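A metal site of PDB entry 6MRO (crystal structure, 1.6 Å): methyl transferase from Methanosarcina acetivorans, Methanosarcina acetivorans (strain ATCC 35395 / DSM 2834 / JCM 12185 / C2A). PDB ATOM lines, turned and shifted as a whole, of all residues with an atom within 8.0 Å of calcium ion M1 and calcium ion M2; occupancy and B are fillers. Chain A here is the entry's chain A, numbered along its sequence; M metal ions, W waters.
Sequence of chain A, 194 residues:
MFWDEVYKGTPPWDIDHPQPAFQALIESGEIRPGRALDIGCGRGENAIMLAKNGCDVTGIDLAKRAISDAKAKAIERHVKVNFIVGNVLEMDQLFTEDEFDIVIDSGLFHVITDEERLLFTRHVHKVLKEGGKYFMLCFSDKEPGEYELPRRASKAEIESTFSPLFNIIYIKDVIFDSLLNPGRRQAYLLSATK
The guanidinium group of Arg 152 sits at hydrogen-bond distance from the backbone carbonyl oxygen of Ser 140, at 2.8 Å. The backbone NH (N) of Asp 141 is in hydrogen-bond range of the backbone carbonyl oxygen (O) of Ala 153 (2.9 Å). N of Glu 157 lies within hydrogen-bond range of OG of Ser 154, 3.0 Å away.
Within 4 Å of calcium ion M2: Asp 141, Glu 143, Gly 145, Glu 146 and Glu 148. The nearest printed residue that does not touch calcium ion M2 is Pro 144 (4.3 Å).
Calcium ion M1 is bound by the backbone carbonyl oxygen (O) of Arg 152 (2.3 Å), the side-chain carboxylate (OD2) of Asp 141 (2.4 Å), water W1 (2.4 Å), the side-chain carboxylate (OE1) of Glu 146 (2.4 Å), water W2 (2.5 Å), the side-chain carboxylate (OE2) of Glu 146 (2.5 Å), the side-chain carboxylate (OE1) of Glu 157 (2.6 Å) and the side-chain carboxylate (OE2) of Glu 157 (2.8 Å).
Calcium ion M2 is bound by the backbone carbonyl oxygen (O) of Gly 145 (2.2 Å), water W3 (2.3 Å), the side-chain carboxylate (OE1) of Glu 148 (2.4 Å), the side-chain carboxylate (OE2) of Glu 146 (2.5 Å), the backbone carbonyl oxygen (O) of Glu 143 (2.5 Å), the side-chain carboxylate (OD2) of Asp 141 (2.5 Å) and the side-chain carboxylate (OD1) of Asp 141 (2.6 Å).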
ATOM      1  N   ARG A 117       6.521  23.771  34.519  1.00  0.00           N
ATOM      2  CA  ARG A 117       6.144  24.327  33.217  1.00  0.00           C
ATOM      3  C   ARG A 117       4.690  24.033  32.860  1.00  0.00           C
ATOM      4  O   ARG A 117       3.984  24.922  32.369  1.00  0.00           O
ATOM      5  CB  ARG A 117       7.083  23.781  32.128  1.00  0.00           C
ATOM      6  CG  ARG A 117       8.419  24.510  32.021  1.00  0.00           C
ATOM      7  CD  ARG A 117       8.772  24.803  30.563  1.00  0.00           C
ATOM      8  NE  ARG A 117      10.161  25.230  30.370  1.00  0.00           N
ATOM      9  CZ  ARG A 117      10.665  26.404  30.765  1.00  0.00           C
ATOM     10  NH1 ARG A 117       9.894  27.275  31.412  1.00  0.00           N
ATOM     11  NH2 ARG A 117      11.934  26.704  30.535  1.00  0.00           N
ATOM     12  N   PHE A 139      15.434  33.965  25.503  1.00  0.00           N
ATOM     13  CA  PHE A 139      16.650  33.758  24.733  1.00  0.00           C
ATOM     14  C   PHE A 139      16.483  32.562  23.809  1.00  0.00           C
ATOM     15  O   PHE A 139      15.863  31.565  24.177  1.00  0.00           O
ATOM     16  CB  PHE A 139      17.837  33.543  25.670  1.00  0.00           C
ATOM     17  CG  PHE A 139      18.149  34.726  26.533  1.00  0.00           C
ATOM     18  CD1 PHE A 139      18.403  35.964  25.975  1.00  0.00           C
ATOM     19  CD2 PHE A 139      18.161  34.603  27.914  1.00  0.00           C
ATOM     20  CE1 PHE A 139      18.674  37.067  26.771  1.00  0.00           C
ATOM     21  CE2 PHE A 139      18.435  35.698  28.715  1.00  0.00           C
ATOM     22  CZ  PHE A 139      18.682  36.933  28.133  1.00  0.00           C
ATOM     23  N   SER A 140      17.029  32.651  22.603  1.00  0.00           N
ATOM     24  CA  SER A 140      16.814  31.623  21.596  1.00  0.00           C
ATOM     25  C   SER A 140      17.887  30.551  21.665  1.00  0.00           C
ATOM     26  O   SER A 140      19.065  30.814  21.959  1.00  0.00           O
ATOM     27  CB  SER A 140      16.777  32.233  20.184  1.00  0.00           C
ATOM     28  OG  SER A 140      17.939  32.975  19.888  1.00  0.00           O
ATOM     29  N   ASP A 141      17.468  29.317  21.383  1.00  0.00           N
ATOM     30  CA  ASP A 141      18.325  28.137  21.397  1.00  0.00           C
ATOM     31  C   ASP A 141      18.266  27.512  20.015  1.00  0.00           C
ATOM     32  O   ASP A 141      17.257  26.901  19.631  1.00  0.00           O
ATOM     33  CB  ASP A 141      17.850  27.158  22.459  1.00  0.00           C
ATOM     34  CG  ASP A 141      18.642  25.868  22.485  1.00  0.00           C
ATOM     35  OD1 ASP A 141      19.572  25.686  21.674  1.00  0.00           O
ATOM     36  OD2 ASP A 141      18.316  25.011  23.341  1.00  0.00           O
ATOM     37  N   LYS A 142      19.352  27.667  19.258  1.00  0.00           N
ATOM     38  CA  LYS A 142      19.480  27.011  17.971  1.00  0.00           C
ATOM     39  C   LYS A 142      20.622  26.007  17.969  1.00  0.00           C
ATOM     40  O   LYS A 142      21.047  25.558  16.898  1.00  0.00           O
ATOM     41  CB  LYS A 142      19.671  28.046  16.855  1.00  0.00           C
ATOM     42  CG  LYS A 142      18.553  29.097  16.810  1.00  0.00           C
ATOM     43  CD  LYS A 142      19.037  30.372  16.137  1.00  0.00           C
ATOM     44  CE  LYS A 142      17.888  31.297  15.788  1.00  0.00           C
ATOM     45  NZ  LYS A 142      18.379  32.488  15.044  1.00  0.00           N
ATOM     46  N   GLU A 143      21.146  25.633  19.156  1.00  0.00           N
ATOM     47  CA  GLU A 143      22.273  24.710  19.155  1.00  0.00           C
ATOM     48  C   GLU A 143      21.821  23.305  19.507  1.00  0.00           C
ATOM     49  O   GLU A 143      21.045  23.130  20.457  1.00  0.00           O
ATOM     50  CB  GLU A 143      23.353  25.175  20.126  1.00  0.00           C
ATOM     51  CG  GLU A 143      24.061  26.429  19.653  1.00  0.00           C
ATOM     52  CD  GLU A 143      25.497  26.167  19.232  1.00  0.00           C
ATOM     53  OE1 GLU A 143      26.033  26.993  18.452  1.00  0.00           O
ATOM     54  OE2 GLU A 143      26.080  25.154  19.669  1.00  0.00           O
ATOM     55  N   PRO A 144      22.292  22.286  18.782  1.00  0.00           N
ATOM     56  CA  PRO A 144      21.853  20.917  19.073  1.00  0.00           C
ATOM     57  C   PRO A 144      22.361  20.450  20.424  1.00  0.00           C
ATOM     58  O   PRO A 144      23.476  20.788  20.846  1.00  0.00           O
ATOM     59  CB  PRO A 144      22.473  20.102  17.926  1.00  0.00           C
ATOM     60  CG  PRO A 144      23.600  20.943  17.408  1.00  0.00           C
ATOM     61  CD  PRO A 144      23.202  22.369  17.631  1.00  0.00           C
ATOM     62  N   GLY A 145      21.530  19.665  21.107  1.00  0.00           N
ATOM     63  CA  GLY A 145      21.840  19.238  22.458  1.00  0.00           C
ATOM     64  C   GLY A 145      21.432  20.281  23.474  1.00  0.00           C
ATOM     65  O   GLY A 145      21.046  21.411  23.148  1.00  0.00           O
ATOM     66  N   GLU A 146      21.516  19.915  24.748  1.00  0.00           N
ATOM     67  CA  GLU A 146      21.055  20.791  25.821  1.00  0.00           C
ATOM     68  C   GLU A 146      22.143  21.023  26.856  1.00  0.00           C
ATOM     69  O   GLU A 146      21.903  20.998  28.068  1.00  0.00           O
ATOM     70  CB  GLU A 146      19.786  20.240  26.459  1.00  0.00           C
ATOM     71  CG  GLU A 146      18.554  20.420  25.591  1.00  0.00           C
ATOM     72  CD  GLU A 146      18.129  21.873  25.492  1.00  0.00           C
ATOM     73  OE1 GLU A 146      17.420  22.355  26.417  1.00  0.00           O
ATOM     74  OE2 GLU A 146      18.505  22.535  24.504  1.00  0.00           O
ATOM     75  N   TYR A 147      23.361  21.275  26.395  1.00  0.00           N
ATOM     76  CA  TYR A 147      24.465  21.567  27.297  1.00  0.00           C
ATOM     77  C   TYR A 147      24.561  23.046  27.684  1.00  0.00           C
ATOM     78  O   TYR A 147      25.318  23.363  28.597  1.00  0.00           O
ATOM     79  CB  TYR A 147      25.798  21.149  26.673  1.00  0.00           C
ATOM     80  CG  TYR A 147      25.815  19.851  25.899  1.00  0.00           C
ATOM     81  CD1 TYR A 147      25.644  19.830  24.528  1.00  0.00           C
ATOM     82  CD2 TYR A 147      26.025  18.642  26.556  1.00  0.00           C
ATOM     83  CE1 TYR A 147      25.685  18.650  23.816  1.00  0.00           C
ATOM     84  CE2 TYR A 147      26.057  17.447  25.849  1.00  0.00           C
ATOM     85  CZ  TYR A 147      25.885  17.462  24.477  1.00  0.00           C
ATOM     86  OH  TYR A 147      25.917  16.284  23.755  1.00  0.00           O
ATOM     87  N   GLU A 148      23.839  23.946  27.019  1.00  0.00           N
ATOM     88  CA  GLU A 148      24.066  25.369  27.252  1.00  0.00           C
ATOM     89  C   GLU A 148      23.489  25.802  28.591  1.00  0.00           C
ATOM     90  O   GLU A 148      22.417  25.356  29.017  1.00  0.00           O
ATOM     91  CB  GLU A 148      23.490  26.208  26.109  1.00  0.00           C
ATOM     92  CG  GLU A 148      22.027  25.984  25.775  1.00  0.00           C
ATOM     93  CD  GLU A 148      21.815  24.847  24.769  1.00  0.00           C
ATOM     94  OE1 GLU A 148      20.713  24.267  24.785  1.00  0.00           O
ATOM     95  OE2 GLU A 148      22.715  24.531  23.965  1.00  0.00           O
ATOM     96  N   PRO A 150      23.023  29.486  30.960  1.00  0.00           N
ATOM     97  CA  PRO A 150      21.640  29.136  31.316  1.00  0.00           C
ATOM     98  C   PRO A 150      20.886  28.451  30.166  1.00  0.00           C
ATOM     99  O   PRO A 150      21.345  28.496  29.026  1.00  0.00           O
ATOM    100  CB  PRO A 150      21.001  30.494  31.626  1.00  0.00           C
ATOM    101  CG  PRO A 150      22.138  31.381  31.952  1.00  0.00           C
ATOM    102  CD  PRO A 150      23.282  30.924  31.122  1.00  0.00           C
ATOM    103  N   ARG A 151      19.755  27.810  30.486  1.00  0.00           N
ATOM    104  CA  ARG A 151      18.900  27.247  29.452  1.00  0.00           C
ATOM    105  C   ARG A 151      18.529  28.316  28.419  1.00  0.00           C
ATOM    106  O   ARG A 151      18.499  29.509  28.727  1.00  0.00           O
ATOM    107  CB  ARG A 151      17.624  26.659  30.050  1.00  0.00           C
ATOM    108  CG  ARG A 151      17.767  25.311  30.716  1.00  0.00           C
ATOM    109  CD  ARG A 151      16.465  24.932  31.429  1.00  0.00           C
ATOM    110  NE  ARG A 151      16.079  25.959  32.394  1.00  0.00           N
ATOM    111  CZ  ARG A 151      14.851  26.115  32.870  1.00  0.00           C
ATOM    112  NH1 ARG A 151      14.600  27.085  33.745  1.00  0.00           N
ATOM    113  NH2 ARG A 151      13.867  25.316  32.480  1.00  0.00           N
ATOM    114  N   ARG A 152      18.262  27.874  27.199  1.00  0.00           N
ATOM    115  CA  ARG A 152      17.675  28.739  26.183  1.00  0.00           C
ATOM    116  C   ARG A 152      16.604  27.930  25.459  1.00  0.00           C
ATOM    117  O   ARG A 152      16.691  26.708  25.370  1.00  0.00           O
ATOM    118  CB  ARG A 152      18.721  29.269  25.175  1.00  0.00           C
ATOM    119  CG  ARG A 152      19.910  30.006  25.819  1.00  0.00           C
ATOM    120  CD  ARG A 152      20.628  30.920  24.809  1.00  0.00           C
ATOM    121  NE  ARG A 152      21.201  30.186  23.671  1.00  0.00           N
ATOM    122  CZ  ARG A 152      22.361  29.544  23.686  1.00  0.00           C
ATOM    123  NH1 ARG A 152      23.107  29.527  24.790  1.00  0.00           N
ATOM    124  NH2 ARG A 152      22.774  28.906  22.594  1.00  0.00           N
ATOM    125  N   ALA A 153      15.586  28.619  24.965  1.00  0.00           N
ATOM    126  CA  ALA A 153      14.406  27.950  24.441  1.00  0.00           C
ATOM    127  C   ALA A 153      14.506  27.846  22.923  1.00  0.00           C
ATOM    128  O   ALA A 153      14.782  28.833  22.243  1.00  0.00           O
ATOM    129  CB  ALA A 153      13.135  28.679  24.853  1.00  0.00           C
ATOM    130  N   SER A 154      14.316  26.631  22.401  1.00  0.00           N
ATOM    131  CA  SER A 154      14.260  26.431  20.959  1.00  0.00           C
ATOM    132  C   SER A 154      12.820  26.603  20.495  1.00  0.00           C
ATOM    133  O   SER A 154      11.890  26.634  21.301  1.00  0.00           O
ATOM    134  CB  SER A 154      14.774  25.051  20.580  1.00  0.00           C
ATOM    135  OG  SER A 154      13.885  24.068  21.080  1.00  0.00           O
ATOM    136  N   LYS A 155      12.629  26.712  19.180  1.00  0.00           N
ATOM    137  CA  LYS A 155      11.259  26.783  18.671  1.00  0.00           C
ATOM    138  C   LYS A 155      10.508  25.498  18.985  1.00  0.00           C
ATOM    139  O   LYS A 155       9.326  25.532  19.328  1.00  0.00           O
ATOM    140  CB  LYS A 155      11.260  27.058  17.171  1.00  0.00           C
ATOM    141  CG  LYS A 155      11.958  28.355  16.811  1.00  0.00           C
ATOM    142  CD  LYS A 155      12.073  28.521  15.303  1.00  0.00           C
ATOM    143  CE  LYS A 155      11.272  29.714  14.847  1.00  0.00           C
ATOM    144  NZ  LYS A 155      12.057  30.503  13.864  1.00  0.00           N
ATOM    145  N   GLU A 157      10.992  23.495  21.586  1.00  0.00           N
ATOM    146  CA  GLU A 157      10.625  23.547  22.991  1.00  0.00           C
ATOM    147  C   GLU A 157       9.453  24.491  23.234  1.00  0.00           C
ATOM    148  O   GLU A 157       8.526  24.165  23.986  1.00  0.00           O
ATOM    149  CB  GLU A 157      11.842  23.966  23.844  1.00  0.00           C
ATOM    150  CG  GLU A 157      12.974  22.944  23.769  1.00  0.00           C
ATOM    151  CD  GLU A 157      14.350  23.507  24.149  1.00  0.00           C
ATOM    152  OE1 GLU A 157      15.284  22.704  24.387  1.00  0.00           O
ATOM    153  OE2 GLU A 157      14.500  24.740  24.208  1.00  0.00           O
HETATM  154 CA    CA M   1      17.067  24.450  25.265  1.00  0.00          CA
HETATM  155 CA    CA M   2      19.982  23.297  22.684  1.00  0.00          CA
HETATM  156  O   HOH W   1      19.081  25.060  26.363  1.00  0.00           O
HETATM  157  O   HOH W   2      15.859  24.659  27.399  1.00  0.00           O
HETATM  158  O   HOH W   3      18.269  22.550  21.286  1.00  0.00           O
